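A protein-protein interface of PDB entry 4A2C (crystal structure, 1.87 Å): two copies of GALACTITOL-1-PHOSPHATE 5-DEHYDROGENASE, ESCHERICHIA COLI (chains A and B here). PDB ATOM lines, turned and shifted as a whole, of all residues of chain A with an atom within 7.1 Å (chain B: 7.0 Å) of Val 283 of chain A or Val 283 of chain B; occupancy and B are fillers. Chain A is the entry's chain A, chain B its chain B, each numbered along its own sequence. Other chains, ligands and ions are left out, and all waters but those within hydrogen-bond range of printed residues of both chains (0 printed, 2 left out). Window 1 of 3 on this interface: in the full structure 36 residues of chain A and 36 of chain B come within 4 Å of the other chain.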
ATOM      1  N   VAL A 243      -1.666  -2.049  13.803  1.00  0.00           N
ATOM      2  CA  VAL A 243      -0.883  -1.922  15.045  1.00  0.00           C
ATOM      3  C   VAL A 243       0.608  -1.777  14.697  1.00  0.00           C
ATOM      4  O   VAL A 243       1.308  -0.910  15.222  1.00  0.00           O
ATOM      5  CB  VAL A 243      -1.094  -3.124  15.991  1.00  0.00           C
ATOM      6  CG1 VAL A 243      -0.063  -3.098  17.143  1.00  0.00           C
ATOM      7  CG2 VAL A 243      -2.538  -3.146  16.517  1.00  0.00           C
ATOM      8  N   VAL A 247       3.278   1.820  14.989  1.00  0.00           N
ATOM      9  CA  VAL A 247       4.595   1.818  15.617  1.00  0.00           C
ATOM     10  C   VAL A 247       5.666   2.301  14.640  1.00  0.00           C
ATOM     11  O   VAL A 247       6.593   3.023  15.030  1.00  0.00           O
ATOM     12  CB  VAL A 247       4.967   0.419  16.159  1.00  0.00           C
ATOM     13  CG1 VAL A 247       6.448   0.384  16.571  1.00  0.00           C
ATOM     14  CG2 VAL A 247       4.064   0.037  17.332  1.00  0.00           C
ATOM     15  N   ALA A 254       5.655   9.580  20.809  1.00  0.00           N
ATOM     16  CA  ALA A 254       4.250   9.598  20.426  1.00  0.00           C
ATOM     17  C   ALA A 254       3.489   8.753  21.442  1.00  0.00           C
ATOM     18  O   ALA A 254       3.995   7.740  21.939  1.00  0.00           O
ATOM     19  CB  ALA A 254       4.058   9.028  19.058  1.00  0.00           C
ATOM     20  N   GLN A 255       2.277   9.189  21.758  1.00  0.00           N
ATOM     21  CA  GLN A 255       1.331   8.355  22.490  1.00  0.00           C
ATOM     22  C   GLN A 255       0.573   7.469  21.502  1.00  0.00           C
ATOM     23  O   GLN A 255       0.193   7.923  20.411  1.00  0.00           O
ATOM     24  CB  GLN A 255       0.346   9.232  23.253  1.00  0.00           C
ATOM     25  CG  GLN A 255       0.964   9.973  24.424  1.00  0.00           C
ATOM     26  CD  GLN A 255       0.029  11.017  24.996  1.00  0.00           C
ATOM     27  OE1 GLN A 255      -0.337  11.979  24.313  1.00  0.00           O
ATOM     28  NE2 GLN A 255      -0.366  10.835  26.260  1.00  0.00           N
ATOM     29  N   LEU A 256       0.325   6.222  21.899  1.00  0.00           N
ATOM     30  CA  LEU A 256      -0.316   5.250  21.028  1.00  0.00           C
ATOM     31  C   LEU A 256      -1.461   4.586  21.766  1.00  0.00           C
ATOM     32  O   LEU A 256      -1.244   3.747  22.647  1.00  0.00           O
ATOM     33  CB  LEU A 256       0.701   4.198  20.607  1.00  0.00           C
ATOM     34  CG  LEU A 256       0.540   3.582  19.219  1.00  0.00           C
ATOM     35  CD1 LEU A 256       1.896   3.468  18.539  1.00  0.00           C
ATOM     36  CD2 LEU A 256      -0.124   2.226  19.309  1.00  0.00           C
ATOM     37  N   ALA A 257      -2.689   4.961  21.412  1.00  0.00           N
ATOM     38  CA  ALA A 257      -3.864   4.396  22.092  1.00  0.00           C
ATOM     39  C   ALA A 257      -4.456   3.291  21.227  1.00  0.00           C
ATOM     40  O   ALA A 257      -4.783   3.513  20.051  1.00  0.00           O
ATOM     41  CB  ALA A 257      -4.905   5.485  22.348  1.00  0.00           C
ATOM     42  N   LEU A 258      -4.584   2.100  21.805  1.00  0.00           N
ATOM     43  CA  LEU A 258      -5.162   0.975  21.099  1.00  0.00           C
ATOM     44  C   LEU A 258      -6.627   0.851  21.511  1.00  0.00           C
ATOM     45  O   LEU A 258      -6.942   0.531  22.673  1.00  0.00           O
ATOM     46  CB  LEU A 258      -4.412  -0.307  21.458  1.00  0.00           C
ATOM     47  CG  LEU A 258      -2.894  -0.270  21.250  1.00  0.00           C
ATOM     48  CD1 LEU A 258      -2.205  -1.461  21.900  1.00  0.00           C
ATOM     49  CD2 LEU A 258      -2.576  -0.200  19.765  1.00  0.00           C
ATOM     50  N   PHE A 273       9.430  -3.902  17.396  1.00  0.00           N
ATOM     51  CA  PHE A 273       9.457  -3.871  18.854  1.00  0.00           C
ATOM     52  C   PHE A 273      10.540  -2.904  19.333  1.00  0.00           C
ATOM     53  O   PHE A 273      10.324  -2.133  20.264  1.00  0.00           O
ATOM     54  CB  PHE A 273       9.732  -5.267  19.428  1.00  0.00           C
ATOM     55  CG  PHE A 273       9.783  -5.307  20.938  1.00  0.00           C
ATOM     56  CD1 PHE A 273       8.624  -5.458  21.686  1.00  0.00           C
ATOM     57  CD2 PHE A 273      10.994  -5.199  21.605  1.00  0.00           C
ATOM     58  CE1 PHE A 273       8.668  -5.485  23.074  1.00  0.00           C
ATOM     59  CE2 PHE A 273      11.051  -5.227  22.995  1.00  0.00           C
ATOM     60  CZ  PHE A 273       9.885  -5.370  23.730  1.00  0.00           C
ATOM     61  N   ILE A 276       9.487   0.686  19.536  1.00  0.00           N
ATOM     62  CA  ILE A 276       8.684   1.069  20.697  1.00  0.00           C
ATOM     63  C   ILE A 276       9.655   1.611  21.739  1.00  0.00           C
ATOM     64  O   ILE A 276       9.445   2.661  22.349  1.00  0.00           O
ATOM     65  CB  ILE A 276       7.945  -0.128  21.323  1.00  0.00           C
ATOM     66  CG1 ILE A 276       6.887  -0.687  20.363  1.00  0.00           C
ATOM     67  CG2 ILE A 276       7.298   0.295  22.636  1.00  0.00           C
ATOM     68  CD1 ILE A 276       6.206  -1.966  20.906  1.00  0.00           C
ATOM     69  N   GLU A 280      10.725   5.654  22.403  1.00  0.00           N
ATOM     70  CA  GLU A 280      10.079   5.832  23.712  1.00  0.00           C
ATOM     71  C   GLU A 280       8.586   6.160  23.594  1.00  0.00           C
ATOM     72  O   GLU A 280       8.071   7.148  24.151  1.00  0.00           O
ATOM     73  CB  GLU A 280      10.840   6.810  24.619  1.00  0.00           C
ATOM     74  CG  GLU A 280      12.241   6.299  24.964  1.00  0.00           C
ATOM     75  CD  GLU A 280      12.981   7.152  25.990  1.00  0.00           C
ATOM     76  OE1 GLU A 280      13.038   8.399  25.824  1.00  0.00           O
ATOM     77  OE2 GLU A 280      13.516   6.574  26.967  1.00  0.00           O
ATOM     78  N   LEU A 281       7.894   5.297  22.868  1.00  0.00           N
ATOM     79  CA  LEU A 281       6.453   5.391  22.743  1.00  0.00           C
ATOM     80  C   LEU A 281       5.817   5.077  24.076  1.00  0.00           C
ATOM     81  O   LEU A 281       6.432   4.462  24.959  1.00  0.00           O
ATOM     82  CB  LEU A 281       5.936   4.386  21.710  1.00  0.00           C
ATOM     83  CG  LEU A 281       6.536   4.503  20.316  1.00  0.00           C
ATOM     84  CD1 LEU A 281       5.727   3.650  19.320  1.00  0.00           C
ATOM     85  CD2 LEU A 281       6.575   5.966  19.884  1.00  0.00           C
ATOM     86  N   THR A 282       4.585   5.546  24.231  1.00  0.00           N
ATOM     87  CA  THR A 282       3.762   5.181  25.363  1.00  0.00           C
ATOM     88  C   THR A 282       2.561   4.543  24.698  1.00  0.00           C
ATOM     89  O   THR A 282       1.861   5.206  23.930  1.00  0.00           O
ATOM     90  CB  THR A 282       3.345   6.426  26.137  1.00  0.00           C
ATOM     91  OG1 THR A 282       4.475   6.903  26.885  1.00  0.00           O
ATOM     92  CG2 THR A 282       2.210   6.111  27.096  1.00  0.00           C
ATOM     93  N   VAL A 283       2.348   3.254  24.937  1.00  0.00           N
ATOM     94  CA  VAL A 283       1.231   2.588  24.314  1.00  0.00           C
ATOM     95  C   VAL A 283       0.114   2.406  25.335  1.00  0.00           C
ATOM     96  O   VAL A 283       0.303   1.798  26.399  1.00  0.00           O
ATOM     97  CB  VAL A 283       1.628   1.248  23.717  1.00  0.00           C
ATOM     98  CG1 VAL A 283       0.403   0.607  23.067  1.00  0.00           C
ATOM     99  CG2 VAL A 283       2.765   1.441  22.688  1.00  0.00           C
ATOM    100  N   ILE A 284      -1.058   2.930  25.003  1.00  0.00           N
ATOM    101  CA  ILE A 284      -2.132   3.036  25.980  1.00  0.00           C
ATOM    102  C   ILE A 284      -3.272   2.121  25.593  1.00  0.00           C
ATOM    103  O   ILE A 284      -3.945   2.372  24.593  1.00  0.00           O
ATOM    104  CB  ILE A 284      -2.666   4.488  26.034  1.00  0.00           C
ATOM    105  CG1 ILE A 284      -1.523   5.488  26.265  1.00  0.00           C
ATOM    106  CG2 ILE A 284      -3.719   4.633  27.096  1.00  0.00           C
ATOM    107  CD1 ILE A 284      -1.947   6.947  26.003  1.00  0.00           C
ATOM    108  N   GLY A 285      -3.468   1.052  26.358  1.00  0.00           N
ATOM    109  CA  GLY A 285      -4.577   0.158  26.092  1.00  0.00           C
ATOM    110  C   GLY A 285      -5.859   0.843  26.532  1.00  0.00           C
ATOM    111  O   GLY A 285      -5.917   1.405  27.635  1.00  0.00           O
ATOM    112  N   VAL B 247       2.523  -8.771  30.343  1.00  0.00           N
ATOM    113  CA  VAL B 247       1.146  -8.406  30.016  1.00  0.00           C
ATOM    114  C   VAL B 247       0.165  -9.369  30.696  1.00  0.00           C
ATOM    115  O   VAL B 247      -0.870  -8.952  31.232  1.00  0.00           O
ATOM    116  CB  VAL B 247       0.905  -8.365  28.508  1.00  0.00           C
ATOM    117  CG1 VAL B 247      -0.604  -8.291  28.205  1.00  0.00           C
ATOM    118  CG2 VAL B 247       1.630  -7.156  27.879  1.00  0.00           C
ATOM    119  N   ALA B 254      -1.882  -1.319  35.127  1.00  0.00           N
ATOM    120  CA  ALA B 254      -0.447  -1.384  35.425  1.00  0.00           C
ATOM    121  C   ALA B 254       0.377  -0.596  34.400  1.00  0.00           C
ATOM    122  O   ALA B 254      -0.032  -0.439  33.250  1.00  0.00           O
ATOM    123  CB  ALA B 254       0.025  -2.818  35.491  1.00  0.00           C
ATOM    124  N   GLN B 255       1.515  -0.073  34.850  1.00  0.00           N
ATOM    125  CA  GLN B 255       2.522   0.519  33.963  1.00  0.00           C
ATOM    126  C   GLN B 255       3.579  -0.523  33.644  1.00  0.00           C
ATOM    127  O   GLN B 255       4.160  -1.109  34.550  1.00  0.00           O
ATOM    128  CB  GLN B 255       3.185   1.699  34.653  1.00  0.00           C
ATOM    129  CG  GLN B 255       2.271   2.875  34.925  1.00  0.00           C
ATOM    130  CD  GLN B 255       3.001   3.974  35.663  1.00  0.00           C
ATOM    131  OE1 GLN B 255       3.414   3.801  36.818  1.00  0.00           O
ATOM    132  NE2 GLN B 255       3.201   5.101  34.989  1.00  0.00           N
ATOM    133  N   LEU B 256       3.818  -0.771  32.360  1.00  0.00           N
ATOM    134  CA  LEU B 256       4.830  -1.734  31.927  1.00  0.00           C
ATOM    135  C   LEU B 256       5.921  -0.990  31.194  1.00  0.00           C
ATOM    136  O   LEU B 256       5.695  -0.488  30.088  1.00  0.00           O
ATOM    137  CB  LEU B 256       4.262  -2.741  30.927  1.00  0.00           C
ATOM    138  CG  LEU B 256       3.785  -4.111  31.371  1.00  0.00           C
ATOM    139  CD1 LEU B 256       2.533  -3.942  32.227  1.00  0.00           C
ATOM    140  CD2 LEU B 256       3.507  -4.989  30.136  1.00  0.00           C
ATOM    141  N   ALA B 257       7.107  -0.941  31.789  1.00  0.00           N
ATOM    142  CA  ALA B 257       8.268  -0.338  31.142  1.00  0.00           C
ATOM    143  C   ALA B 257       9.101  -1.401  30.450  1.00  0.00           C
ATOM    144  O   ALA B 257       9.574  -2.357  31.090  1.00  0.00           O
ATOM    145  CB  ALA B 257       9.109   0.404  32.169  1.00  0.00           C
ATOM    146  N   LEU B 258       9.261  -1.260  29.135  1.00  0.00           N
ATOM    147  CA  LEU B 258      10.099  -2.182  28.387  1.00  0.00           C
ATOM    148  C   LEU B 258      11.520  -1.625  28.353  1.00  0.00           C
ATOM    149  O   LEU B 258      11.779  -0.562  27.765  1.00  0.00           O
ATOM    150  CB  LEU B 258       9.571  -2.351  26.958  1.00  0.00           C
ATOM    151  CG  LEU B 258       8.102  -2.746  26.912  1.00  0.00           C
ATOM    152  CD1 LEU B 258       7.603  -2.789  25.472  1.00  0.00           C
ATOM    153  CD2 LEU B 258       7.903  -4.095  27.601  1.00  0.00           C
ATOM    154  N   PHE B 273      -2.493  -9.735  23.370  1.00  0.00           N
ATOM    155  CA  PHE B 273      -2.669  -8.357  22.931  1.00  0.00           C
ATOM    156  C   PHE B 273      -3.965  -7.808  23.522  1.00  0.00           C
ATOM    157  O   PHE B 273      -4.007  -6.666  23.987  1.00  0.00           O
ATOM    158  CB  PHE B 273      -2.714  -8.264  21.403  1.00  0.00           C
ATOM    159  CG  PHE B 273      -3.098  -6.898  20.890  1.00  0.00           C
ATOM    160  CD1 PHE B 273      -4.434  -6.552  20.730  1.00  0.00           C
ATOM    161  CD2 PHE B 273      -2.128  -5.965  20.572  1.00  0.00           C
ATOM    162  CE1 PHE B 273      -4.793  -5.303  20.263  1.00  0.00           C
ATOM    163  CE2 PHE B 273      -2.478  -4.704  20.097  1.00  0.00           C
ATOM    164  CZ  PHE B 273      -3.816  -4.374  19.941  1.00  0.00           C
ATOM    165  N   ILE B 276      -3.816  -6.038  26.864  1.00  0.00           N
ATOM    166  CA  ILE B 276      -3.289  -4.687  27.008  1.00  0.00           C
ATOM    167  C   ILE B 276      -4.481  -3.713  26.991  1.00  0.00           C
ATOM    168  O   ILE B 276      -4.568  -2.789  27.799  1.00  0.00           O
ATOM    169  CB  ILE B 276      -2.265  -4.326  25.928  1.00  0.00           C
ATOM    170  CG1 ILE B 276      -1.098  -5.327  25.960  1.00  0.00           C
ATOM    171  CG2 ILE B 276      -1.750  -2.887  26.161  1.00  0.00           C
ATOM    172  CD1 ILE B 276      -0.315  -5.424  24.660  1.00  0.00           C
ATOM    173  N   GLU B 280      -6.401  -1.943  30.455  1.00  0.00           N
ATOM    174  CA  GLU B 280      -5.957  -0.568  30.185  1.00  0.00           C
ATOM    175  C   GLU B 280      -4.503  -0.325  30.670  1.00  0.00           C
ATOM    176  O   GLU B 280      -4.186   0.621  31.404  1.00  0.00           O
ATOM    177  CB  GLU B 280      -6.962   0.467  30.714  1.00  0.00           C
ATOM    178  CG  GLU B 280      -8.268   0.538  29.857  1.00  0.00           C
ATOM    179  CD  GLU B 280      -9.276   1.556  30.355  1.00  0.00           C
ATOM    180  OE1 GLU B 280      -9.405   1.735  31.588  1.00  0.00           O
ATOM    181  OE2 GLU B 280      -9.966   2.179  29.517  1.00  0.00           O
ATOM    182  N   LEU B 281      -3.610  -1.186  30.219  1.00  0.00           N
ATOM    183  CA  LEU B 281      -2.199  -1.045  30.548  1.00  0.00           C
ATOM    184  C   LEU B 281      -1.613   0.200  29.884  1.00  0.00           C
ATOM    185  O   LEU B 281      -2.102   0.638  28.845  1.00  0.00           O
ATOM    186  CB  LEU B 281      -1.430  -2.270  30.062  1.00  0.00           C
ATOM    187  CG  LEU B 281      -1.778  -3.623  30.674  1.00  0.00           C
ATOM    188  CD1 LEU B 281      -0.797  -4.711  30.250  1.00  0.00           C
ATOM    189  CD2 LEU B 281      -1.860  -3.540  32.204  1.00  0.00           C
ATOM    190  N   THR B 282      -0.576   0.776  30.491  1.00  0.00           N
ATOM    191  CA  THR B 282       0.246   1.759  29.781  1.00  0.00           C
ATOM    192  C   THR B 282       1.609   1.117  29.560  1.00  0.00           C
ATOM    193  O   THR B 282       2.315   0.779  30.515  1.00  0.00           O
ATOM    194  CB  THR B 282       0.468   3.038  30.583  1.00  0.00           C
ATOM    195  OG1 THR B 282      -0.779   3.696  30.798  1.00  0.00           O
ATOM    196  CG2 THR B 282       1.405   3.992  29.802  1.00  0.00           C
ATOM    197  N   VAL B 283       1.982   0.933  28.303  1.00  0.00           N
ATOM    198  CA  VAL B 283       3.242   0.292  28.005  1.00  0.00           C
ATOM    199  C   VAL B 283       4.256   1.329  27.551  1.00  0.00           C
ATOM    200  O   VAL B 283       4.061   2.036  26.548  1.00  0.00           O
ATOM    201  CB  VAL B 283       3.099  -0.779  26.940  1.00  0.00           C
ATOM    202  CG1 VAL B 283       4.475  -1.403  26.668  1.00  0.00           C
ATOM    203  CG2 VAL B 283       2.118  -1.838  27.417  1.00  0.00           C
ATOM    204  N   ILE B 284       5.351   1.396  28.296  1.00  0.00           N
ATOM    205  CA  ILE B 284       6.274   2.500  28.199  1.00  0.00           C
ATOM    206  C   ILE B 284       7.585   2.025  27.588  1.00  0.00           C
ATOM    207  O   ILE B 284       8.340   1.319  28.235  1.00  0.00           O
ATOM    208  CB  ILE B 284       6.520   3.067  29.622  1.00  0.00           C
ATOM    209  CG1 ILE B 284       5.191   3.506  30.263  1.00  0.00           C
ATOM    210  CG2 ILE B 284       7.517   4.208  29.591  1.00  0.00           C
ATOM    211  CD1 ILE B 284       5.289   3.896  31.736  1.00  0.00           C
ATOM    212  N   GLY B 285       7.860   2.375  26.335  1.00  0.00           N
ATOM    213  CA  GLY B 285       9.165   2.032  25.779  1.00  0.00           C
ATOM    214  C   GLY B 285      10.234   2.845  26.489  1.00  0.00           C
ATOM    215  O   GLY B 285      10.090   4.059  26.621  1.00  0.00           O
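The backbone NH of Gly 285 of chain B sits at hydrogen-bond distance from the backbone carbonyl oxygen of Leu 281 of chain A (2.9 Å).
The backbone carbonyl oxygen (O) of Val 283 of chain B lies within hydrogen-bond range of the backbone NH (N) of Val 283 of chain A, 2.6 Å away.
O of Leu 281 of chain B is in hydrogen-bond range of N of Gly 285 of chain A (2.9 Å).
N of Thr 282 of chain A lies within hydrogen-bond range of O of Ala 254 of chain A, 3.2 Å away.
The backbone NH of Leu 256 of chain A is in hydrogen-bond range of the backbone carbonyl oxygen of Thr 282 of chain A.
O of Ile 276 of chain A lies within hydrogen-bond range of N of Leu 281 of chain A (3.1 Å).
The backbone carbonyl oxygen of Ala 254 of chain B sits at hydrogen-bond distance from the backbone NH of Thr 282 of chain B, at 3.1 Å.
O of Leu 256 of chain B sits at hydrogen-bond distance from N of Ile 284 of chain B, at 2.6 Å.
O of Ile 284 of chain B is in hydrogen-bond range of N of Leu 258 of chain B (2.9 Å).
Among the printed residues, pairs that only touch across the chains: Val 243 of chain A with Phe 273 of chain B, Leu 258 of chain A with Phe 273 of chain B, Phe 273 of chain A with Leu 258 of chain B, Ile 276 of chain A with Gly 285 of chain B, Glu 280 of chain A with Gly 285 of chain B, Leu 281 of chain A with Val 283 of chain B, Leu 281 of chain A with Ile 284 of chain B, Thr 282 of chain A with Thr 282 of chain B, Thr 282 of chain A with Val 283 of chain B, Val 283 of chain A with Leu 281 of chain B, Val 283 of chain A with Thr 282 of chain B, Ile 284 of chain A with Leu 281 of chain B, Gly 285 of chain A with Ile 276 of chain B and Gly 285 of chain A with Glu 280 of chain B.
Of chain A, only Leu 281 (3.7 Å), Thr 282 (3.4 Å) and Val 283 (2.6 Å) come within 4 Å of Val 283 of chain B.
Of the printed residues of chain A, Glu 280 of chain B touches Gly 285.
Of the printed residues of chain B, Ile 284 of chain A touches Leu 281 (3.7 Å).
Val 247 of chain A touches none of the printed residues of chain B.
Hydrophobic or aromatic side chains of chain A that line the printed part of chain B: Val 243, Leu 258, Phe 273 and Val 283.
Leu 258 of chain A touches Phe 273 of chain B, and with the chains exchanged Phe 273 of chain A touches Leu 258 of chain B.
Ile 276 of chain A touches Gly 285 of chain B, and with the chains exchanged Gly 285 of chain A touches Ile 276 of chain B.
Leu 281 of chain A touches Val 283 of chain B, and with the chains exchanged Val 283 of chain A touches Leu 281 of chain B.
Thr 282 of chain A touches Val 283 of chain B, and with the chains exchanged Val 283 of chain A touches Thr 282 of chain B.
Of the 17 pairs that touch across the chains among the printed residues, 16 have their exchanged pair printed and touching as well.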
